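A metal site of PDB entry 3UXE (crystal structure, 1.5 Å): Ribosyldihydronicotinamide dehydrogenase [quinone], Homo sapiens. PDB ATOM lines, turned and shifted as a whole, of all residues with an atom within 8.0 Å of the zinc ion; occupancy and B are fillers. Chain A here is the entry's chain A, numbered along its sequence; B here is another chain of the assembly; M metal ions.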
ATOM      1  N   TYR A 132       6.620  22.310  18.399  1.00  0.00           N
ATOM      2  CA  TYR A 132       5.902  22.084  17.104  1.00  0.00           C
ATOM      3  C   TYR A 132       4.725  22.989  16.975  1.00  0.00           C
ATOM      4  O   TYR A 132       4.906  24.202  16.925  1.00  0.00           O
ATOM      5  CB  TYR A 132       5.555  20.555  16.831  1.00  0.00           C
ATOM      6  CG  TYR A 132       6.811  19.677  16.566  1.00  0.00           C
ATOM      7  CD1 TYR A 132       7.698  19.946  15.505  1.00  0.00           C
ATOM      8  CD2 TYR A 132       7.175  18.699  17.467  1.00  0.00           C
ATOM      9  CE1 TYR A 132       8.842  19.168  15.287  1.00  0.00           C
ATOM     10  CE2 TYR A 132       8.351  17.925  17.290  1.00  0.00           C
ATOM     11  CZ  TYR A 132       9.172  18.186  16.178  1.00  0.00           C
ATOM     12  OH  TYR A 132      10.335  17.471  15.895  1.00  0.00           O
ATOM     13  N   ASP A 133       3.499  22.463  16.964  1.00  0.00           N
ATOM     14  CA  ASP A 133       2.374  23.432  16.695  1.00  0.00           C
ATOM     15  C   ASP A 133       2.133  24.305  17.911  1.00  0.00           C
ATOM     16  O   ASP A 133       1.511  25.351  17.808  1.00  0.00           O
ATOM     17  CB  ASP A 133       1.094  22.683  16.295  1.00  0.00           C
ATOM     18  CG  ASP A 133       1.161  22.206  14.866  1.00  0.00           C
ATOM     19  OD1 ASP A 133       2.186  22.483  14.201  1.00  0.00           O
ATOM     20  OD2 ASP A 133       0.215  21.526  14.442  1.00  0.00           O
ATOM     21  N   TRP A 169      15.053  17.805   6.324  1.00  0.00           N
ATOM     22  CA  TRP A 169      14.333  17.379   7.521  1.00  0.00           C
ATOM     23  C   TRP A 169      14.811  18.012   8.807  1.00  0.00           C
ATOM     24  O   TRP A 169      13.984  18.617   9.493  1.00  0.00           O
ATOM     25  CB  TRP A 169      14.269  15.832   7.567  1.00  0.00           C
ATOM     26  CG  TRP A 169      13.693  15.227   8.782  1.00  0.00           C
ATOM     27  CD1 TRP A 169      14.372  14.606   9.858  1.00  0.00           C
ATOM     28  CD2 TRP A 169      12.309  15.130   9.083  1.00  0.00           C
ATOM     29  NE1 TRP A 169      13.424  14.069  10.723  1.00  0.00           N
ATOM     30  CE2 TRP A 169      12.174  14.442  10.325  1.00  0.00           C
ATOM     31  CE3 TRP A 169      11.148  15.598   8.439  1.00  0.00           C
ATOM     32  CZ2 TRP A 169      10.926  14.133  10.886  1.00  0.00           C
ATOM     33  CZ3 TRP A 169       9.909  15.339   9.033  1.00  0.00           C
ATOM     34  CH2 TRP A 169       9.814  14.572  10.244  1.00  0.00           C
ATOM     35  N   LEU A 171      16.408  20.769   9.343  1.00  0.00           N
ATOM     36  CA  LEU A 171      16.252  22.220   9.309  1.00  0.00           C
ATOM     37  C   LEU A 171      14.752  22.577   9.259  1.00  0.00           C
ATOM     38  O   LEU A 171      14.358  23.396  10.086  1.00  0.00           O
ATOM     39  CB  LEU A 171      16.961  22.778   8.040  1.00  0.00           C
ATOM     40  CG  LEU A 171      18.489  22.427   8.032  1.00  0.00           C
ATOM     41  CD1 LEU A 171      19.024  22.708   6.611  1.00  0.00           C
ATOM     42  CD2 LEU A 171      19.194  23.237   9.081  1.00  0.00           C
ATOM     43  N   GLN A 172      13.981  22.010   8.309  1.00  0.00           N
ATOM     44  CA  GLN A 172      12.596  22.420   8.216  1.00  0.00           C
ATOM     45  C   GLN A 172      11.786  21.824   9.377  1.00  0.00           C
ATOM     46  O   GLN A 172      11.002  22.604  10.019  1.00  0.00           O
ATOM     47  CB  GLN A 172      12.007  21.946   6.876  1.00  0.00           C
ATOM     48  CG  GLN A 172      12.635  22.671   5.711  1.00  0.00           C
ATOM     49  CD  GLN A 172      11.954  22.447   4.416  1.00  0.00           C
ATOM     50  OE1 GLN A 172      11.303  21.381   4.207  1.00  0.00           O
ATOM     51  NE2 GLN A 172      12.125  23.374   3.488  1.00  0.00           N
ATOM     52  N   HIS A 173      11.893  20.516   9.661  1.00  0.00           N
ATOM     53  CA  HIS A 173      11.076  19.913  10.681  1.00  0.00           C
ATOM     54  C   HIS A 173      11.614  20.048  12.074  1.00  0.00           C
ATOM     55  O   HIS A 173      10.982  20.611  12.971  1.00  0.00           O
ATOM     56  CB  HIS A 173      10.762  18.448  10.326  1.00  0.00           C
ATOM     57  CG  HIS A 173       9.851  17.788  11.322  1.00  0.00           C
ATOM     58  ND1 HIS A 173       8.494  17.979  11.317  1.00  0.00           N
ATOM     59  CD2 HIS A 173      10.113  17.026  12.404  1.00  0.00           C
ATOM     60  CE1 HIS A 173       7.943  17.290  12.302  1.00  0.00           C
ATOM     61  NE2 HIS A 173       8.908  16.709  12.992  1.00  0.00           N
ATOM     62  N   GLY A 174      12.881  19.612  12.267  1.00  0.00           N
ATOM     63  CA  GLY A 174      13.439  19.596  13.653  1.00  0.00           C
ATOM     64  C   GLY A 174      13.707  20.982  14.220  1.00  0.00           C
ATOM     65  O   GLY A 174      13.858  21.102  15.443  1.00  0.00           O
ATOM     66  N   THR A 175      13.924  21.947  13.296  1.00  0.00           N
ATOM     67  CA  THR A 175      14.225  23.340  13.720  1.00  0.00           C
ATOM     68  C   THR A 175      13.062  24.281  13.533  1.00  0.00           C
ATOM     69  O   THR A 175      12.432  24.685  14.570  1.00  0.00           O
ATOM     70  CB  THR A 175      15.512  23.893  13.095  1.00  0.00           C
ATOM     71  OG1 THR A 175      16.565  22.892  13.329  1.00  0.00           O
ATOM     72  CG2 THR A 175      15.895  25.167  13.695  1.00  0.00           C
ATOM     73  N   LEU A 176      12.734  24.592  12.248  1.00  0.00           N
ATOM     74  CA  LEU A 176      11.690  25.650  11.980  1.00  0.00           C
ATOM     75  C   LEU A 176      10.316  25.186  12.479  1.00  0.00           C
ATOM     76  O   LEU A 176       9.652  25.923  13.179  1.00  0.00           O
ATOM     77  CB  LEU A 176      11.704  25.947  10.469  1.00  0.00           C
ATOM     78  CG  LEU A 176      13.093  26.544  10.047  1.00  0.00           C
ATOM     79  CD1 LEU A 176      13.028  26.793   8.536  1.00  0.00           C
ATOM     80  CD2 LEU A 176      13.395  27.831  10.824  1.00  0.00           C
ATOM     81  N   HIS A 177       9.863  23.969  12.155  1.00  0.00           N
ATOM     82  CA  HIS A 177       8.524  23.560  12.629  1.00  0.00           C
ATOM     83  C   HIS A 177       8.508  23.440  14.145  1.00  0.00           C
ATOM     84  O   HIS A 177       7.466  23.708  14.811  1.00  0.00           O
ATOM     85  CB  HIS A 177       8.145  22.296  11.908  1.00  0.00           C
ATOM     86  CG  HIS A 177       6.745  21.791  12.205  1.00  0.00           C
ATOM     87  ND1 HIS A 177       6.278  20.590  11.744  1.00  0.00           N
ATOM     88  CD2 HIS A 177       5.727  22.363  12.873  1.00  0.00           C
ATOM     89  CE1 HIS A 177       5.039  20.417  12.131  1.00  0.00           C
ATOM     90  NE2 HIS A 177       4.667  21.495  12.820  1.00  0.00           N
ATOM     91  N   PHE A 178       9.593  22.947  14.719  1.00  0.00           N
ATOM     92  CA  PHE A 178       9.617  22.786  16.172  1.00  0.00           C
ATOM     93  C   PHE A 178       9.348  24.065  16.915  1.00  0.00           C
ATOM     94  O   PHE A 178       8.683  24.096  17.966  1.00  0.00           O
ATOM     95  CB  PHE A 178      10.925  22.177  16.608  1.00  0.00           C
ATOM     96  CG  PHE A 178      11.037  21.892  18.057  1.00  0.00           C
ATOM     97  CD1 PHE A 178      10.706  20.626  18.529  1.00  0.00           C
ATOM     98  CD2 PHE A 178      11.615  22.809  18.973  1.00  0.00           C
ATOM     99  CE1 PHE A 178      10.847  20.300  19.879  1.00  0.00           C
ATOM    100  CE2 PHE A 178      11.769  22.496  20.357  1.00  0.00           C
ATOM    101  CZ  PHE A 178      11.387  21.186  20.792  1.00  0.00           C
ATOM    102  N   PHE A 181       7.153  27.735  13.364  1.00  0.00           N
ATOM    103  CA  PHE A 181       7.058  28.379  12.062  1.00  0.00           C
ATOM    104  C   PHE A 181       6.244  27.482  11.143  1.00  0.00           C
ATOM    105  O   PHE A 181       6.292  26.219  11.256  1.00  0.00           O
ATOM    106  CB  PHE A 181       8.394  28.468  11.360  1.00  0.00           C
ATOM    107  CG  PHE A 181       9.377  29.555  11.859  1.00  0.00           C
ATOM    108  CD1 PHE A 181       9.283  30.884  11.380  1.00  0.00           C
ATOM    109  CD2 PHE A 181      10.421  29.219  12.756  1.00  0.00           C
ATOM    110  CE1 PHE A 181      10.217  31.840  11.748  1.00  0.00           C
ATOM    111  CE2 PHE A 181      11.374  30.212  13.142  1.00  0.00           C
ATOM    112  CZ  PHE A 181      11.226  31.567  12.607  1.00  0.00           C
ATOM    113  N   VAL A 183       6.378  26.745   7.202  1.00  0.00           N
ATOM    114  CA  VAL A 183       7.543  26.621   6.309  1.00  0.00           C
ATOM    115  C   VAL A 183       7.188  26.732   4.831  1.00  0.00           C
ATOM    116  O   VAL A 183       6.463  25.869   4.330  1.00  0.00           O
ATOM    117  CB  VAL A 183       8.276  25.232   6.558  1.00  0.00           C
ATOM    118  CG1 VAL A 183       9.462  25.080   5.550  1.00  0.00           C
ATOM    119  CG2 VAL A 183       8.805  25.243   8.014  1.00  0.00           C
ATOM    120  N   ILE A 220       4.193  24.463   3.216  1.00  0.00           N
ATOM    121  CA  ILE A 220       4.218  22.997   2.987  1.00  0.00           C
ATOM    122  C   ILE A 220       3.662  22.321   4.194  1.00  0.00           C
ATOM    123  O   ILE A 220       3.695  22.884   5.318  1.00  0.00           O
ATOM    124  CB  ILE A 220       5.631  22.449   2.737  1.00  0.00           C
ATOM    125  CG1 ILE A 220       6.521  22.549   3.978  1.00  0.00           C
ATOM    126  CG2 ILE A 220       6.267  23.075   1.525  1.00  0.00           C
ATOM    127  CD1 ILE A 220       7.829  21.750   3.848  1.00  0.00           C
ATOM    128  N   PRO A 221       3.101  21.096   3.991  1.00  0.00           N
ATOM    129  CA  PRO A 221       2.819  20.277   5.169  1.00  0.00           C
ATOM    130  C   PRO A 221       4.139  19.692   5.688  1.00  0.00           C
ATOM    131  O   PRO A 221       4.732  18.818   5.012  1.00  0.00           O
ATOM    132  CB  PRO A 221       1.896  19.186   4.624  1.00  0.00           C
ATOM    133  CG  PRO A 221       2.149  19.094   3.107  1.00  0.00           C
ATOM    134  CD  PRO A 221       2.516  20.559   2.733  1.00  0.00           C
ATOM    135  N   CYS A 222       4.657  20.250   6.789  1.00  0.00           N
ATOM    136  CA  CYS A 222       5.985  19.867   7.268  1.00  0.00           C
ATOM    137  C   CYS A 222       5.904  18.554   8.099  1.00  0.00           C
ATOM    138  O   CYS A 222       6.036  18.519   9.369  1.00  0.00           O
ATOM    139  CB  CYS A 222       6.612  21.007   8.065  1.00  0.00           C
ATOM    140  SG  CYS A 222       8.322  20.665   8.661  1.00  0.00           S
ATOM    141  N   THR A 223       5.733  17.500   7.344  1.00  0.00           N
ATOM    142  CA  THR A 223       5.507  16.191   7.893  1.00  0.00           C
ATOM    143  C   THR A 223       6.587  15.224   7.370  1.00  0.00           C
ATOM    144  O   THR A 223       7.253  15.501   6.390  1.00  0.00           O
ATOM    145  CB  THR A 223       4.110  15.670   7.450  1.00  0.00           C
ATOM    146  OG1 THR A 223       4.087  15.573   6.022  1.00  0.00           O
ATOM    147  CG2 THR A 223       2.993  16.573   7.956  1.00  0.00           C
ATOM    148  N   ALA A 224       6.749  14.075   8.050  1.00  0.00           N
ATOM    149  CA  ALA A 224       7.635  13.010   7.548  1.00  0.00           C
ATOM    150  C   ALA A 224       7.225  12.548   6.119  1.00  0.00           C
ATOM    151  O   ALA A 224       8.076  12.266   5.258  1.00  0.00           O
ATOM    152  CB  ALA A 224       7.596  11.774   8.523  1.00  0.00           C
ATOM    153  N   TRP A 226       5.941  14.420   3.650  1.00  0.00           N
ATOM    154  CA  TRP A 226       6.387  15.365   2.661  1.00  0.00           C
ATOM    155  C   TRP A 226       7.893  15.121   2.359  1.00  0.00           C
ATOM    156  O   TRP A 226       8.326  15.150   1.189  1.00  0.00           O
ATOM    157  CB  TRP A 226       6.172  16.796   3.165  1.00  0.00           C
ATOM    158  CG  TRP A 226       6.511  17.860   2.144  1.00  0.00           C
ATOM    159  CD1 TRP A 226       5.648  18.449   1.258  1.00  0.00           C
ATOM    160  CD2 TRP A 226       7.806  18.442   1.892  1.00  0.00           C
ATOM    161  NE1 TRP A 226       6.327  19.354   0.481  1.00  0.00           N
ATOM    162  CE2 TRP A 226       7.645  19.378   0.838  1.00  0.00           C
ATOM    163  CE3 TRP A 226       9.088  18.279   2.471  1.00  0.00           C
ATOM    164  CZ2 TRP A 226       8.722  20.144   0.340  1.00  0.00           C
ATOM    165  CZ3 TRP A 226      10.156  19.039   1.972  1.00  0.00           C
ATOM    166  CH2 TRP A 226       9.956  19.977   0.905  1.00  0.00           C
ATOM    167  N   HIS A 227       8.674  14.853   3.415  1.00  0.00           N
ATOM    168  CA  HIS A 227      10.120  14.732   3.235  1.00  0.00           C
ATOM    169  C   HIS A 227      10.574  13.364   2.680  1.00  0.00           C
ATOM    170  O   HIS A 227      11.553  13.295   1.910  1.00  0.00           O
ATOM    171  CB  HIS A 227      10.861  14.990   4.560  1.00  0.00           C
ATOM    172  CG  HIS A 227      10.798  16.430   5.011  1.00  0.00           C
ATOM    173  ND1 HIS A 227       9.694  16.968   5.662  1.00  0.00           N
ATOM    174  CD2 HIS A 227      11.733  17.417   4.951  1.00  0.00           C
ATOM    175  CE1 HIS A 227       9.960  18.243   5.955  1.00  0.00           C
ATOM    176  NE2 HIS A 227      11.183  18.535   5.531  1.00  0.00           N
ATOM    177  N   VAL B 160       6.427  12.377  17.319  1.00  0.00           N
ATOM    178  CA  VAL B 160       6.538  13.787  16.849  1.00  0.00           C
ATOM    179  C   VAL B 160       7.864  14.155  16.177  1.00  0.00           C
ATOM    180  O   VAL B 160       7.875  15.053  15.273  1.00  0.00           O
ATOM    181  CB  VAL B 160       6.239  14.817  18.006  1.00  0.00           C
ATOM    182  CG1 VAL B 160       4.752  14.758  18.405  1.00  0.00           C
ATOM    183  CG2 VAL B 160       7.203  14.669  19.238  1.00  0.00           C
HETATM  184 ZN    ZN M   1       7.483  19.488  10.356  1.00  0.00          ZN
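Within 4 Å of the zinc ion: His 173, His 177 and Cys 222.
The backbone carbonyl oxygen (O) of Cys 222 binds the zinc ion. ND1 of His 173 binds the zinc ion (2.1 Å). The zinc ion is bound by ND1 of His 177, at 2.1 Å. SG of Cys 222 binds the zinc ion (2.2 Å).
O of Gln 172 lies close to SG of Cys 222 (3.6 Å). A ring nitrogen (NE2) of His 173 sits at hydrogen-bond distance from the backbone carbonyl oxygen (O) of Val 160 of chain B (3.0 Å). A ring nitrogen (NE2) of His 177 sits at hydrogen-bond distance from the side-chain carboxylate (OD1) of Asp 133, at 3.0 Å. A ring nitrogen (NE2) of His 173 sits at hydrogen-bond distance from the side-chain hydroxyl (OH) of Tyr 132 (3.3 Å). N of His 177 lies within hydrogen-bond range of O of Gln 172 (2.8 Å). The backbone carbonyl oxygen of His 173 sits at hydrogen-bond distance from the backbone NH of Phe 178, at 3.2 Å.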
